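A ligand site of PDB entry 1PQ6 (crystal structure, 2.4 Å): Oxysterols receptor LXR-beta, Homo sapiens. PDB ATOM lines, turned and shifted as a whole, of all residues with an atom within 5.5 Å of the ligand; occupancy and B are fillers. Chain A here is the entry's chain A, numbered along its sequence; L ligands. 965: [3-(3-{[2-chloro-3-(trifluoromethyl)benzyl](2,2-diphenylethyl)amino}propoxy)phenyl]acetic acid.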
ATOM      1  N   ASN A  31     -14.679  20.171   5.863  1.00  0.00           N
ATOM      2  CA  ASN A  31     -16.055  20.556   6.042  1.00  0.00           C
ATOM      3  C   ASN A  31     -17.026  19.540   5.415  1.00  0.00           C
ATOM      4  O   ASN A  31     -17.945  19.065   6.083  1.00  0.00           O
ATOM      5  CB  ASN A  31     -16.236  21.938   5.425  1.00  0.00           C
ATOM      6  CG  ASN A  31     -17.607  22.508   5.685  1.00  0.00           C
ATOM      7  OD1 ASN A  31     -17.943  22.837   6.838  1.00  0.00           O
ATOM      8  ND2 ASN A  31     -18.412  22.637   4.625  1.00  0.00           N
ATOM      9  N   PHE A  60     -26.641  22.354  26.675  1.00  0.00           N
ATOM     10  CA  PHE A  60     -25.215  22.379  26.896  1.00  0.00           C
ATOM     11  C   PHE A  60     -24.530  21.118  26.360  1.00  0.00           C
ATOM     12  O   PHE A  60     -23.480  21.202  25.765  1.00  0.00           O
ATOM     13  CB  PHE A  60     -24.894  22.553  28.386  1.00  0.00           C
ATOM     14  CG  PHE A  60     -23.417  22.597  28.683  1.00  0.00           C
ATOM     15  CD1 PHE A  60     -22.651  23.694  28.284  1.00  0.00           C
ATOM     16  CD2 PHE A  60     -22.787  21.525  29.304  1.00  0.00           C
ATOM     17  CE1 PHE A  60     -21.306  23.728  28.538  1.00  0.00           C
ATOM     18  CE2 PHE A  60     -21.420  21.562  29.547  1.00  0.00           C
ATOM     19  CZ  PHE A  60     -20.691  22.674  29.179  1.00  0.00           C
ATOM     20  N   PHE A  63     -24.340  21.496  22.505  1.00  0.00           N
ATOM     21  CA  PHE A  63     -23.354  22.422  21.953  1.00  0.00           C
ATOM     22  C   PHE A  63     -21.931  21.927  22.148  1.00  0.00           C
ATOM     23  O   PHE A  63     -21.054  22.142  21.344  1.00  0.00           O
ATOM     24  CB  PHE A  63     -23.446  23.752  22.677  1.00  0.00           C
ATOM     25  CG  PHE A  63     -24.503  24.683  22.163  1.00  0.00           C
ATOM     26  CD1 PHE A  63     -24.880  24.698  20.828  1.00  0.00           C
ATOM     27  CD2 PHE A  63     -25.087  25.600  23.030  1.00  0.00           C
ATOM     28  CE1 PHE A  63     -25.843  25.589  20.381  1.00  0.00           C
ATOM     29  CE2 PHE A  63     -26.034  26.507  22.583  1.00  0.00           C
ATOM     30  CZ  PHE A  63     -26.408  26.500  21.248  1.00  0.00           C
ATOM     31  N   THR A  64     -21.722  21.300  23.290  1.00  0.00           N
ATOM     32  CA  THR A  64     -20.517  20.538  23.598  1.00  0.00           C
ATOM     33  C   THR A  64     -20.209  19.522  22.488  1.00  0.00           C
ATOM     34  O   THR A  64     -19.073  19.384  22.058  1.00  0.00           O
ATOM     35  CB  THR A  64     -20.695  19.873  25.001  1.00  0.00           C
ATOM     36  OG1 THR A  64     -19.572  20.158  25.815  1.00  0.00           O
ATOM     37  CG2 THR A  64     -20.778  18.340  24.976  1.00  0.00           C
ATOM     38  N   LEU A  66     -21.440  19.630  19.275  1.00  0.00           N
ATOM     39  CA  LEU A  66     -21.122  20.375  18.052  1.00  0.00           C
ATOM     40  C   LEU A  66     -19.660  20.852  18.069  1.00  0.00           C
ATOM     41  O   LEU A  66     -18.987  20.870  17.044  1.00  0.00           O
ATOM     42  CB  LEU A  66     -22.071  21.586  17.861  1.00  0.00           C
ATOM     43  CG  LEU A  66     -23.540  21.257  17.636  1.00  0.00           C
ATOM     44  CD1 LEU A  66     -24.409  22.489  17.721  1.00  0.00           C
ATOM     45  CD2 LEU A  66     -23.750  20.598  16.304  1.00  0.00           C
ATOM     46  N   ALA A  67     -19.176  21.216  19.262  1.00  0.00           N
ATOM     47  CA  ALA A  67     -17.820  21.709  19.443  1.00  0.00           C
ATOM     48  C   ALA A  67     -16.793  20.605  19.255  1.00  0.00           C
ATOM     49  O   ALA A  67     -15.718  20.844  18.741  1.00  0.00           O
ATOM     50  CB  ALA A  67     -17.670  22.371  20.838  1.00  0.00           C
ATOM     51  N   ILE A  69     -17.269  18.081  17.161  1.00  0.00           N
ATOM     52  CA  ILE A  69     -17.281  17.939  15.705  1.00  0.00           C
ATOM     53  C   ILE A  69     -16.272  18.930  15.129  1.00  0.00           C
ATOM     54  O   ILE A  69     -15.450  18.569  14.304  1.00  0.00           O
ATOM     55  CB  ILE A  69     -18.651  18.261  15.075  1.00  0.00           C
ATOM     56  CG1 ILE A  69     -19.762  17.296  15.494  1.00  0.00           C
ATOM     57  CG2 ILE A  69     -18.512  18.284  13.543  1.00  0.00           C
ATOM     58  CD1 ILE A  69     -19.411  15.885  15.423  1.00  0.00           C
ATOM     59  N   SER A  70     -16.371  20.180  15.546  1.00  0.00           N
ATOM     60  CA  SER A  70     -15.457  21.229  15.042  1.00  0.00           C
ATOM     61  C   SER A  70     -14.014  20.928  15.397  1.00  0.00           C
ATOM     62  O   SER A  70     -13.130  21.162  14.592  1.00  0.00           O
ATOM     63  CB  SER A  70     -15.854  22.613  15.598  1.00  0.00           C
ATOM     64  OG  SER A  70     -14.756  23.504  15.623  1.00  0.00           O
ATOM     65  N   GLU A  73     -12.674  18.514  12.850  1.00  0.00           N
ATOM     66  CA  GLU A  73     -12.338  19.221  11.618  1.00  0.00           C
ATOM     67  C   GLU A  73     -11.011  19.941  11.710  1.00  0.00           C
ATOM     68  O   GLU A  73     -10.177  19.797  10.855  1.00  0.00           O
ATOM     69  CB  GLU A  73     -13.377  20.274  11.298  1.00  0.00           C
ATOM     70  CG  GLU A  73     -14.726  19.726  10.948  1.00  0.00           C
ATOM     71  CD  GLU A  73     -15.655  20.831  10.550  1.00  0.00           C
ATOM     72  OE1 GLU A  73     -16.725  20.959  11.187  1.00  0.00           O
ATOM     73  OE2 GLU A  73     -15.315  21.585   9.586  1.00  0.00           O
ATOM     74  N   ILE A 101      -9.446  26.742  20.106  1.00  0.00           N
ATOM     75  CA  ILE A 101     -10.547  27.648  20.457  1.00  0.00           C
ATOM     76  C   ILE A 101     -10.571  28.846  19.490  1.00  0.00           C
ATOM     77  O   ILE A 101     -11.629  29.284  19.060  1.00  0.00           O
ATOM     78  CB  ILE A 101     -10.482  28.092  21.957  1.00  0.00           C
ATOM     79  CG1 ILE A 101     -11.745  28.835  22.364  1.00  0.00           C
ATOM     80  CG2 ILE A 101      -9.269  29.012  22.236  1.00  0.00           C
ATOM     81  CD1 ILE A 101     -12.889  27.937  22.652  1.00  0.00           C
ATOM     82  N   MET A 104     -11.976  27.870  16.116  1.00  0.00           N
ATOM     83  CA  MET A 104     -13.385  27.643  16.325  1.00  0.00           C
ATOM     84  C   MET A 104     -14.116  28.947  16.289  1.00  0.00           C
ATOM     85  O   MET A 104     -15.192  28.981  15.759  1.00  0.00           O
ATOM     86  CB  MET A 104     -13.663  26.999  17.682  1.00  0.00           C
ATOM     87  CG  MET A 104     -13.369  25.565  17.775  1.00  0.00           C
ATOM     88  SD  MET A 104     -14.046  24.740  19.269  1.00  0.00           S
ATOM     89  CE  MET A 104     -15.682  25.191  19.207  1.00  0.00           C
ATOM     90  N   LEU A 105     -13.553  29.978  16.906  1.00  0.00           N
ATOM     91  CA  LEU A 105     -14.196  31.286  16.925  1.00  0.00           C
ATOM     92  C   LEU A 105     -14.215  31.841  15.527  1.00  0.00           C
ATOM     93  O   LEU A 105     -15.211  32.427  15.107  1.00  0.00           O
ATOM     94  CB  LEU A 105     -13.471  32.270  17.847  1.00  0.00           C
ATOM     95  CG  LEU A 105     -13.671  31.989  19.333  1.00  0.00           C
ATOM     96  CD1 LEU A 105     -12.556  32.646  20.110  1.00  0.00           C
ATOM     97  CD2 LEU A 105     -15.024  32.470  19.807  1.00  0.00           C
ATOM     98  N   GLU A 107     -14.319  30.046  12.780  1.00  0.00           N
ATOM     99  CA  GLU A 107     -15.326  29.238  12.055  1.00  0.00           C
ATOM    100  C   GLU A 107     -16.747  29.654  12.455  1.00  0.00           C
ATOM    101  O   GLU A 107     -17.691  29.666  11.638  1.00  0.00           O
ATOM    102  CB  GLU A 107     -15.108  27.723  12.295  1.00  0.00           C
ATOM    103  CG  GLU A 107     -13.945  27.088  11.537  1.00  0.00           C
ATOM    104  CD  GLU A 107     -14.035  27.300  10.028  1.00  0.00           C
ATOM    105  OE1 GLU A 107     -14.841  26.606   9.378  1.00  0.00           O
ATOM    106  OE2 GLU A 107     -13.330  28.208   9.501  1.00  0.00           O
ATOM    107  N   THR A 108     -16.896  30.020  13.718  1.00  0.00           N
ATOM    108  CA  THR A 108     -18.170  30.485  14.208  1.00  0.00           C
ATOM    109  C   THR A 108     -18.513  31.828  13.591  1.00  0.00           C
ATOM    110  O   THR A 108     -19.654  32.055  13.225  1.00  0.00           O
ATOM    111  CB  THR A 108     -18.115  30.594  15.724  1.00  0.00           C
ATOM    112  OG1 THR A 108     -17.929  29.291  16.277  1.00  0.00           O
ATOM    113  CG2 THR A 108     -19.465  31.135  16.305  1.00  0.00           C
ATOM    114  N   ARG A 111     -19.989  31.468  10.171  1.00  0.00           N
ATOM    115  CA  ARG A 111     -21.344  30.901  10.163  1.00  0.00           C
ATOM    116  C   ARG A 111     -22.403  31.818  10.763  1.00  0.00           C
ATOM    117  O   ARG A 111     -23.566  31.419  10.938  1.00  0.00           O
ATOM    118  CB  ARG A 111     -21.357  29.586  10.937  1.00  0.00           C
ATOM    119  CG  ARG A 111     -20.626  28.471  10.262  1.00  0.00           C
ATOM    120  CD  ARG A 111     -20.171  27.385  11.203  1.00  0.00           C
ATOM    121  NE  ARG A 111     -19.664  26.238  10.471  1.00  0.00           N
ATOM    122  CZ  ARG A 111     -18.491  26.193   9.865  1.00  0.00           C
ATOM    123  NH1 ARG A 111     -17.680  27.229   9.917  1.00  0.00           N
ATOM    124  NH2 ARG A 111     -18.122  25.099   9.207  1.00  0.00           N
ATOM    125  N   ILE A 119     -26.398  31.906  14.209  1.00  0.00           N
ATOM    126  CA  ILE A 119     -25.205  31.168  13.835  1.00  0.00           C
ATOM    127  C   ILE A 119     -25.611  29.747  13.450  1.00  0.00           C
ATOM    128  O   ILE A 119     -26.352  29.109  14.198  1.00  0.00           O
ATOM    129  CB  ILE A 119     -24.228  31.125  15.023  1.00  0.00           C
ATOM    130  CG1 ILE A 119     -23.637  32.515  15.260  1.00  0.00           C
ATOM    131  CG2 ILE A 119     -23.137  30.115  14.807  1.00  0.00           C
ATOM    132  CD1 ILE A 119     -22.933  32.619  16.584  1.00  0.00           C
ATOM    133  N   THR A 120     -25.100  29.252  12.326  1.00  0.00           N
ATOM    134  CA  THR A 120     -25.498  27.956  11.785  1.00  0.00           C
ATOM    135  C   THR A 120     -24.347  26.948  11.766  1.00  0.00           C
ATOM    136  O   THR A 120     -23.342  27.125  11.058  1.00  0.00           O
ATOM    137  CB  THR A 120     -26.091  28.116  10.373  1.00  0.00           C
ATOM    138  OG1 THR A 120     -27.221  29.001  10.406  1.00  0.00           O
ATOM    139  CG2 THR A 120     -26.701  26.789   9.853  1.00  0.00           C
ATOM    140  N   PHE A 121     -24.513  25.889  12.556  1.00  0.00           N
ATOM    141  CA  PHE A 121     -23.595  24.762  12.554  1.00  0.00           C
ATOM    142  C   PHE A 121     -24.112  23.643  11.649  1.00  0.00           C
ATOM    143  O   PHE A 121     -25.313  23.370  11.600  1.00  0.00           O
ATOM    144  CB  PHE A 121     -23.410  24.280  14.001  1.00  0.00           C
ATOM    145  CG  PHE A 121     -23.043  25.390  14.953  1.00  0.00           C
ATOM    146  CD1 PHE A 121     -23.887  25.731  16.001  1.00  0.00           C
ATOM    147  CD2 PHE A 121     -21.862  26.112  14.772  1.00  0.00           C
ATOM    148  CE1 PHE A 121     -23.569  26.767  16.859  1.00  0.00           C
ATOM    149  CE2 PHE A 121     -21.522  27.152  15.639  1.00  0.00           C
ATOM    150  CZ  PHE A 121     -22.382  27.477  16.688  1.00  0.00           C
ATOM    151  N   LEU A 122     -23.205  23.034  10.882  1.00  0.00           N
ATOM    152  CA  LEU A 122     -23.489  21.781  10.153  1.00  0.00           C
ATOM    153  C   LEU A 122     -24.671  21.855   9.164  1.00  0.00           C
ATOM    154  O   LEU A 122     -25.517  20.960   9.137  1.00  0.00           O
ATOM    155  CB  LEU A 122     -23.741  20.639  11.160  1.00  0.00           C
ATOM    156  CG  LEU A 122     -22.617  20.308  12.144  1.00  0.00           C
ATOM    157  CD1 LEU A 122     -23.126  19.422  13.252  1.00  0.00           C
ATOM    158  CD2 LEU A 122     -21.464  19.639  11.448  1.00  0.00           C
ATOM    159  N   PHE A 132     -27.894  30.509  23.227  1.00  0.00           N
ATOM    160  CA  PHE A 132     -26.638  30.307  23.937  1.00  0.00           C
ATOM    161  C   PHE A 132     -26.788  30.592  25.425  1.00  0.00           C
ATOM    162  O   PHE A 132     -26.142  29.941  26.246  1.00  0.00           O
ATOM    163  CB  PHE A 132     -25.483  31.116  23.312  1.00  0.00           C
ATOM    164  CG  PHE A 132     -25.149  30.687  21.913  1.00  0.00           C
ATOM    165  CD1 PHE A 132     -25.559  31.429  20.816  1.00  0.00           C
ATOM    166  CD2 PHE A 132     -24.428  29.529  21.692  1.00  0.00           C
ATOM    167  CE1 PHE A 132     -25.266  31.021  19.528  1.00  0.00           C
ATOM    168  CE2 PHE A 132     -24.116  29.115  20.403  1.00  0.00           C
ATOM    169  CZ  PHE A 132     -24.535  29.861  19.316  1.00  0.00           C
ATOM    170  N   LEU A 137     -24.396  29.441  29.312  1.00  0.00           N
ATOM    171  CA  LEU A 137     -23.148  30.147  29.078  1.00  0.00           C
ATOM    172  C   LEU A 137     -23.224  31.569  29.657  1.00  0.00           C
ATOM    173  O   LEU A 137     -24.259  32.221  29.556  1.00  0.00           O
ATOM    174  CB  LEU A 137     -22.808  30.134  27.579  1.00  0.00           C
ATOM    175  CG  LEU A 137     -22.735  28.741  26.929  1.00  0.00           C
ATOM    176  CD1 LEU A 137     -22.668  28.856  25.427  1.00  0.00           C
ATOM    177  CD2 LEU A 137     -21.543  27.953  27.429  1.00  0.00           C
ATOM    178  N   PHE A 141     -19.275  35.773  28.016  1.00  0.00           N
ATOM    179  CA  PHE A 141     -18.695  34.890  26.997  1.00  0.00           C
ATOM    180  C   PHE A 141     -19.429  35.095  25.690  1.00  0.00           C
ATOM    181  O   PHE A 141     -18.819  35.262  24.660  1.00  0.00           O
ATOM    182  CB  PHE A 141     -18.879  33.447  27.484  1.00  0.00           C
ATOM    183  CG  PHE A 141     -18.267  32.402  26.612  1.00  0.00           C
ATOM    184  CD1 PHE A 141     -16.920  32.431  26.285  1.00  0.00           C
ATOM    185  CD2 PHE A 141     -19.031  31.324  26.148  1.00  0.00           C
ATOM    186  CE1 PHE A 141     -16.366  31.455  25.502  1.00  0.00           C
ATOM    187  CE2 PHE A 141     -18.473  30.327  25.376  1.00  0.00           C
ATOM    188  CZ  PHE A 141     -17.136  30.391  25.058  1.00  0.00           C
ATOM    189  N   ILE A 142     -20.758  35.107  25.754  1.00  0.00           N
ATOM    190  CA  ILE A 142     -21.604  35.221  24.576  1.00  0.00           C
ATOM    191  C   ILE A 142     -21.459  36.545  23.836  1.00  0.00           C
ATOM    192  O   ILE A 142     -21.371  36.575  22.617  1.00  0.00           O
ATOM    193  CB  ILE A 142     -23.077  35.039  24.967  1.00  0.00           C
ATOM    194  CG1 ILE A 142     -23.371  33.570  25.280  1.00  0.00           C
ATOM    195  CG2 ILE A 142     -23.991  35.553  23.864  1.00  0.00           C
ATOM    196  CD1 ILE A 142     -24.631  33.344  26.144  1.00  0.00           C
ATOM    197  N   ILE A 145     -18.302  36.998  21.768  1.00  0.00           N
ATOM    198  CA  ILE A 145     -18.211  36.127  20.581  1.00  0.00           C
ATOM    199  C   ILE A 145     -19.088  36.691  19.465  1.00  0.00           C
ATOM    200  O   ILE A 145     -18.717  36.615  18.308  1.00  0.00           O
ATOM    201  CB  ILE A 145     -18.655  34.655  20.872  1.00  0.00           C
ATOM    202  CG1 ILE A 145     -17.764  33.931  21.885  1.00  0.00           C
ATOM    203  CG2 ILE A 145     -18.723  33.886  19.578  1.00  0.00           C
ATOM    204  CD1 ILE A 145     -16.443  34.583  22.202  1.00  0.00           C
ATOM    205  N   PHE A 146     -20.256  37.227  19.817  1.00  0.00           N
ATOM    206  CA  PHE A 146     -21.147  37.890  18.837  1.00  0.00           C
ATOM    207  C   PHE A 146     -20.590  39.221  18.296  1.00  0.00           C
ATOM    208  O   PHE A 146     -20.806  39.529  17.120  1.00  0.00           O
ATOM    209  CB  PHE A 146     -22.545  38.116  19.385  1.00  0.00           C
ATOM    210  CG  PHE A 146     -23.467  36.997  19.091  1.00  0.00           C
ATOM    211  CD1 PHE A 146     -23.512  35.888  19.927  1.00  0.00           C
ATOM    212  CD2 PHE A 146     -24.276  37.029  17.976  1.00  0.00           C
ATOM    213  CE1 PHE A 146     -24.366  34.811  19.648  1.00  0.00           C
ATOM    214  CE2 PHE A 146     -25.146  35.967  17.697  1.00  0.00           C
ATOM    215  CZ  PHE A 146     -25.191  34.858  18.533  1.00  0.00           C
ATOM    216  N   HIS A 227     -12.559  32.599  27.188  1.00  0.00           N
ATOM    217  CA  HIS A 227     -12.921  31.208  27.181  1.00  0.00           C
ATOM    218  C   HIS A 227     -12.372  30.426  28.404  1.00  0.00           C
ATOM    219  O   HIS A 227     -13.083  29.617  28.967  1.00  0.00           O
ATOM    220  CB  HIS A 227     -12.455  30.570  25.885  1.00  0.00           C
ATOM    221  CG  HIS A 227     -12.534  29.079  25.869  1.00  0.00           C
ATOM    222  ND1 HIS A 227     -11.415  28.282  25.822  1.00  0.00           N
ATOM    223  CD2 HIS A 227     -13.604  28.233  25.880  1.00  0.00           C
ATOM    224  CE1 HIS A 227     -11.788  27.011  25.809  1.00  0.00           C
ATOM    225  NE2 HIS A 227     -13.100  26.953  25.865  1.00  0.00           N
ATOM    226  N   GLN A 230     -14.567  31.088  31.095  1.00  0.00           N
ATOM    227  CA  GLN A 230     -15.851  30.372  30.970  1.00  0.00           C
ATOM    228  C   GLN A 230     -15.666  28.900  31.361  1.00  0.00           C
ATOM    229  O   GLN A 230     -16.566  28.283  31.904  1.00  0.00           O
ATOM    230  CB  GLN A 230     -16.462  30.539  29.568  1.00  0.00           C
ATOM    231  CG  GLN A 230     -17.635  29.588  29.208  1.00  0.00           C
ATOM    232  CD  GLN A 230     -18.891  29.834  30.019  1.00  0.00           C
ATOM    233  OE1 GLN A 230     -19.792  30.567  29.588  1.00  0.00           O
ATOM    234  NE2 GLN A 230     -18.969  29.204  31.185  1.00  0.00           N
ATOM    235  N   VAL A 231     -14.473  28.362  31.128  1.00  0.00           N
ATOM    236  CA  VAL A 231     -14.181  26.988  31.488  1.00  0.00           C
ATOM    237  C   VAL A 231     -14.089  26.872  33.003  1.00  0.00           C
ATOM    238  O   VAL A 231     -14.549  25.902  33.582  1.00  0.00           O
ATOM    239  CB  VAL A 231     -12.868  26.499  30.836  1.00  0.00           C
ATOM    240  CG1 VAL A 231     -12.402  25.200  31.486  1.00  0.00           C
ATOM    241  CG2 VAL A 231     -13.068  26.305  29.372  1.00  0.00           C
ATOM    242  N   LEU A 234     -17.474  26.903  34.578  1.00  0.00           N
ATOM    243  CA  LEU A 234     -18.127  25.596  34.471  1.00  0.00           C
ATOM    244  C   LEU A 234     -17.683  24.675  35.605  1.00  0.00           C
ATOM    245  O   LEU A 234     -18.501  24.012  36.207  1.00  0.00           O
ATOM    246  CB  LEU A 234     -17.841  24.933  33.125  1.00  0.00           C
ATOM    247  CG  LEU A 234     -18.401  25.623  31.897  1.00  0.00           C
ATOM    248  CD1 LEU A 234     -17.867  24.964  30.639  1.00  0.00           C
ATOM    249  CD2 LEU A 234     -19.921  25.645  31.899  1.00  0.00           C
ATOM    250  N   LEU A 241     -16.975  19.312  31.101  1.00  0.00           N
ATOM    251  CA  LEU A 241     -16.633  19.114  29.701  1.00  0.00           C
ATOM    252  C   LEU A 241     -16.564  17.618  29.407  1.00  0.00           C
ATOM    253  O   LEU A 241     -16.054  16.854  30.209  1.00  0.00           O
ATOM    254  CB  LEU A 241     -15.274  19.723  29.386  1.00  0.00           C
ATOM    255  CG  LEU A 241     -15.167  21.216  29.591  1.00  0.00           C
ATOM    256  CD1 LEU A 241     -13.784  21.654  29.233  1.00  0.00           C
ATOM    257  CD2 LEU A 241     -16.192  21.935  28.755  1.00  0.00           C
ATOM    258  N   LEU A 245     -13.156  17.348  24.874  1.00  0.00           N
ATOM    259  CA  LEU A 245     -12.905  18.756  25.197  1.00  0.00           C
ATOM    260  C   LEU A 245     -12.091  18.904  26.484  1.00  0.00           C
ATOM    261  O   LEU A 245     -11.240  19.779  26.572  1.00  0.00           O
ATOM    262  CB  LEU A 245     -14.226  19.513  25.336  1.00  0.00           C
ATOM    263  CG  LEU A 245     -15.015  19.525  24.041  1.00  0.00           C
ATOM    264  CD1 LEU A 245     -16.300  20.316  24.246  1.00  0.00           C
ATOM    265  CD2 LEU A 245     -14.155  20.086  22.890  1.00  0.00           C
ATOM    266  N   TRP A 249      -8.907  21.607  27.406  1.00  0.00           N
ATOM    267  CA  TRP A 249      -9.162  22.836  28.143  1.00  0.00           C
ATOM    268  C   TRP A 249      -9.118  22.790  29.666  1.00  0.00           C
ATOM    269  O   TRP A 249      -8.960  23.847  30.301  1.00  0.00           O
ATOM    270  CB  TRP A 249     -10.507  23.394  27.691  1.00  0.00           C
ATOM    271  CG  TRP A 249     -10.497  23.734  26.261  1.00  0.00           C
ATOM    272  CD1 TRP A 249      -9.439  24.156  25.518  1.00  0.00           C
ATOM    273  CD2 TRP A 249     -11.616  23.708  25.374  1.00  0.00           C
ATOM    274  NE1 TRP A 249      -9.827  24.378  24.214  1.00  0.00           N
ATOM    275  CE2 TRP A 249     -11.157  24.103  24.101  1.00  0.00           C
ATOM    276  CE3 TRP A 249     -12.967  23.382  25.515  1.00  0.00           C
ATOM    277  CZ2 TRP A 249     -11.994  24.176  22.985  1.00  0.00           C
ATOM    278  CZ3 TRP A 249     -13.803  23.455  24.409  1.00  0.00           C
ATOM    279  CH2 TRP A 249     -13.302  23.847  23.154  1.00  0.00           C
HETATM  280  O37 965 L   1     -20.885  23.552  12.429  1.00  0.00           O
HETATM  281  C35 965 L   1     -19.848  23.075  11.961  1.00  0.00           C
HETATM  282  O36 965 L   1     -19.736  22.810  10.745  1.00  0.00           O
HETATM  283  C34 965 L   1     -18.649  22.731  12.791  1.00  0.00           C
HETATM  284  C32 965 L   1     -18.502  23.708  13.951  1.00  0.00           C
HETATM  285  C31 965 L   1     -17.816  24.897  13.721  1.00  0.00           C
HETATM  286  C30 965 L   1     -17.702  25.855  14.723  1.00  0.00           C
HETATM  287  C29 965 L   1     -18.283  25.628  15.965  1.00  0.00           C
HETATM  288  C28 965 L   1     -18.978  24.442  16.194  1.00  0.00           C
HETATM  289  O27 965 L   1     -19.512  24.229  17.423  1.00  0.00           O
HETATM  290  C26 965 L   1     -20.427  25.137  17.986  1.00  0.00           C
HETATM  291  C25 965 L   1     -20.464  24.925  19.461  1.00  0.00           C
HETATM  292  C17 965 L   1     -21.170  26.085  20.142  1.00  0.00           C
HETATM  293  N09 965 L   1     -20.478  26.463  21.374  1.00  0.00           N
HETATM  294  C16 965 L   1     -20.066  25.412  22.285  1.00  0.00           C
HETATM  295  C18 965 L   1     -18.725  25.641  22.901  1.00  0.00           C
HETATM  296  C23 965 L   1     -17.618  25.992  22.160  1.00  0.00           C
HETATM  297  C22 965 L   1     -16.391  26.198  22.792  1.00  0.00           C
HETATM  298  C21 965 L   1     -16.226  26.058  24.174  1.00  0.00           C
HETATM  299  C20 965 L   1     -17.291  25.698  25.004  1.00  0.00           C
HETATM  300  C19 965 L   1     -18.601  25.467  24.357  1.00  0.00           C
HETATM  301 CL4  965 L   1     -20.025  25.008  25.329  1.00  0.00          CL
HETATM  302  C39 965 L   1     -17.187  25.556  26.509  1.00  0.00           C
HETATM  303  F41 965 L   1     -17.991  26.476  27.046  1.00  0.00           F
HETATM  304  F40 965 L   1     -15.946  25.701  26.923  1.00  0.00           F
HETATM  305  F42 965 L   1     -17.596  24.355  26.896  1.00  0.00           F
HETATM  306  C08 965 L   1     -20.530  27.839  21.863  1.00  0.00           C
HETATM  307  C07 965 L   1     -20.209  28.912  20.805  1.00  0.00           C
HETATM  308  C01 965 L   1     -20.782  30.238  21.152  1.00  0.00           C
HETATM  309  C02 965 L   1     -20.936  30.673  22.482  1.00  0.00           C
HETATM  310  C03 965 L   1     -21.484  31.923  22.771  1.00  0.00           C
HETATM  311  C04 965 L   1     -21.890  32.764  21.749  1.00  0.00           C
HETATM  312  C05 965 L   1     -21.756  32.326  20.440  1.00  0.00           C
HETATM  313  C06 965 L   1     -21.193  31.091  20.129  1.00  0.00           C
HETATM  314  C10 965 L   1     -18.733  29.022  20.629  1.00  0.00           C
HETATM  315  C15 965 L   1     -17.914  29.356  21.706  1.00  0.00           C
HETATM  316  C14 965 L   1     -16.524  29.433  21.545  1.00  0.00           C
HETATM  317  C13 965 L   1     -15.977  29.204  20.276  1.00  0.00           C
HETATM  318  C12 965 L   1     -16.814  28.877  19.220  1.00  0.00           C
HETATM  319  C11 965 L   1     -18.188  28.784  19.391  1.00  0.00           C
HETATM  320  C33 965 L   1     -19.095  23.475  15.193  1.00  0.00           C
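The backbone carbonyl oxygen (O) of Leu 66 sits close to an oxygen (O27) of the ligand (3.4 Å).
A fluorine (F40) of the ligand sits close to a ring nitrogen (NE2) of His 227 (3.3 Å).
CE1 of Phe 60 touches CL4 of the ligand, at 3.7 Å.
Phe 63 touches the ligand (O to C25, 3.4 Å).
Ala 67 touches the ligand.
Ser 70 touches the ligand.
Glu 73 touches the ligand (OE1 to C34, 3.1 Å).
Ile 101 touches the ligand.
CE of Met 104 touches C23 of the ligand, at 3.6 Å.
Leu 105 touches the ligand.
Thr 108 touches the ligand (OG1 to C11, 3.2 Å).
CA of Phe 121 touches O37 of the ligand, 3.0 Å away.
Phe 132 touches the ligand (CE2 to C06, 3.5 Å).
Leu 137 touches the ligand.
Phe 141 touches the ligand.
Ile 142 touches the ligand.
Ile 145 touches the ligand (CG2 to C05, 3.5 Å).
Phe 146 touches the ligand (CE1 to C05, 3.7 Å).
Gln 230 touches the ligand.
Val 231 touches the ligand.
Leu 234 touches the ligand.
Leu 241 touches the ligand (CD2 to F42, 3.4 Å).
Trp 249 touches the ligand.
Hydrophobic or aromatic side chains that line the ligand: Phe 60, Phe 63, Leu 66, Ala 67, Ile 101, Met 104, Leu 105, Phe 121, Leu 122, Phe 132, Leu 137, Phe 141, Ile 142, Ile 145, Phe 146, His 227, Val 231, Leu 234, Leu 241 and Trp 249.
Within 4 Å of the ligand: Phe 60, Phe 63, Leu 66, Ala 67, Ser 70, Glu 73, Ile 101, Met 104, Leu 105, Thr 108, Arg 111, Phe 121, Leu 122, Phe 132, Leu 137, Phe 141, Ile 142, Ile 145, Phe 146, His 227, Gln 230, Val 231, Leu 234, Leu 241 and Trp 249.
The nearest printed residue that does not touch the ligand is Glu 107 (4.01 Å).
The backbone NH (N) of Leu 122 lies within hydrogen-bond range of an oxygen (O37) of the ligand (2.8 Å).
O36 of the ligand lies within salt-bridge range of NH2 of Arg 111, 3.2 Å away.
The backbone carbonyl oxygen (O) of Met 104 is in hydrogen-bond range of the side-chain hydroxyl (OG1) of Thr 108, at 2.8 Å.
NH1 of Arg 111 lies within salt-bridge range of OE1 of Glu 107, 3.0 Å away.
The side-chain amide oxygen (OD1) of Asn 31 lies within hydrogen-bond range of the guanidinium group (NH2) of Arg 111, at 3.3 Å.
The backbone NH of Thr 120 sits at hydrogen-bond distance from the backbone carbonyl oxygen of Arg 111, at 3.0 Å.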
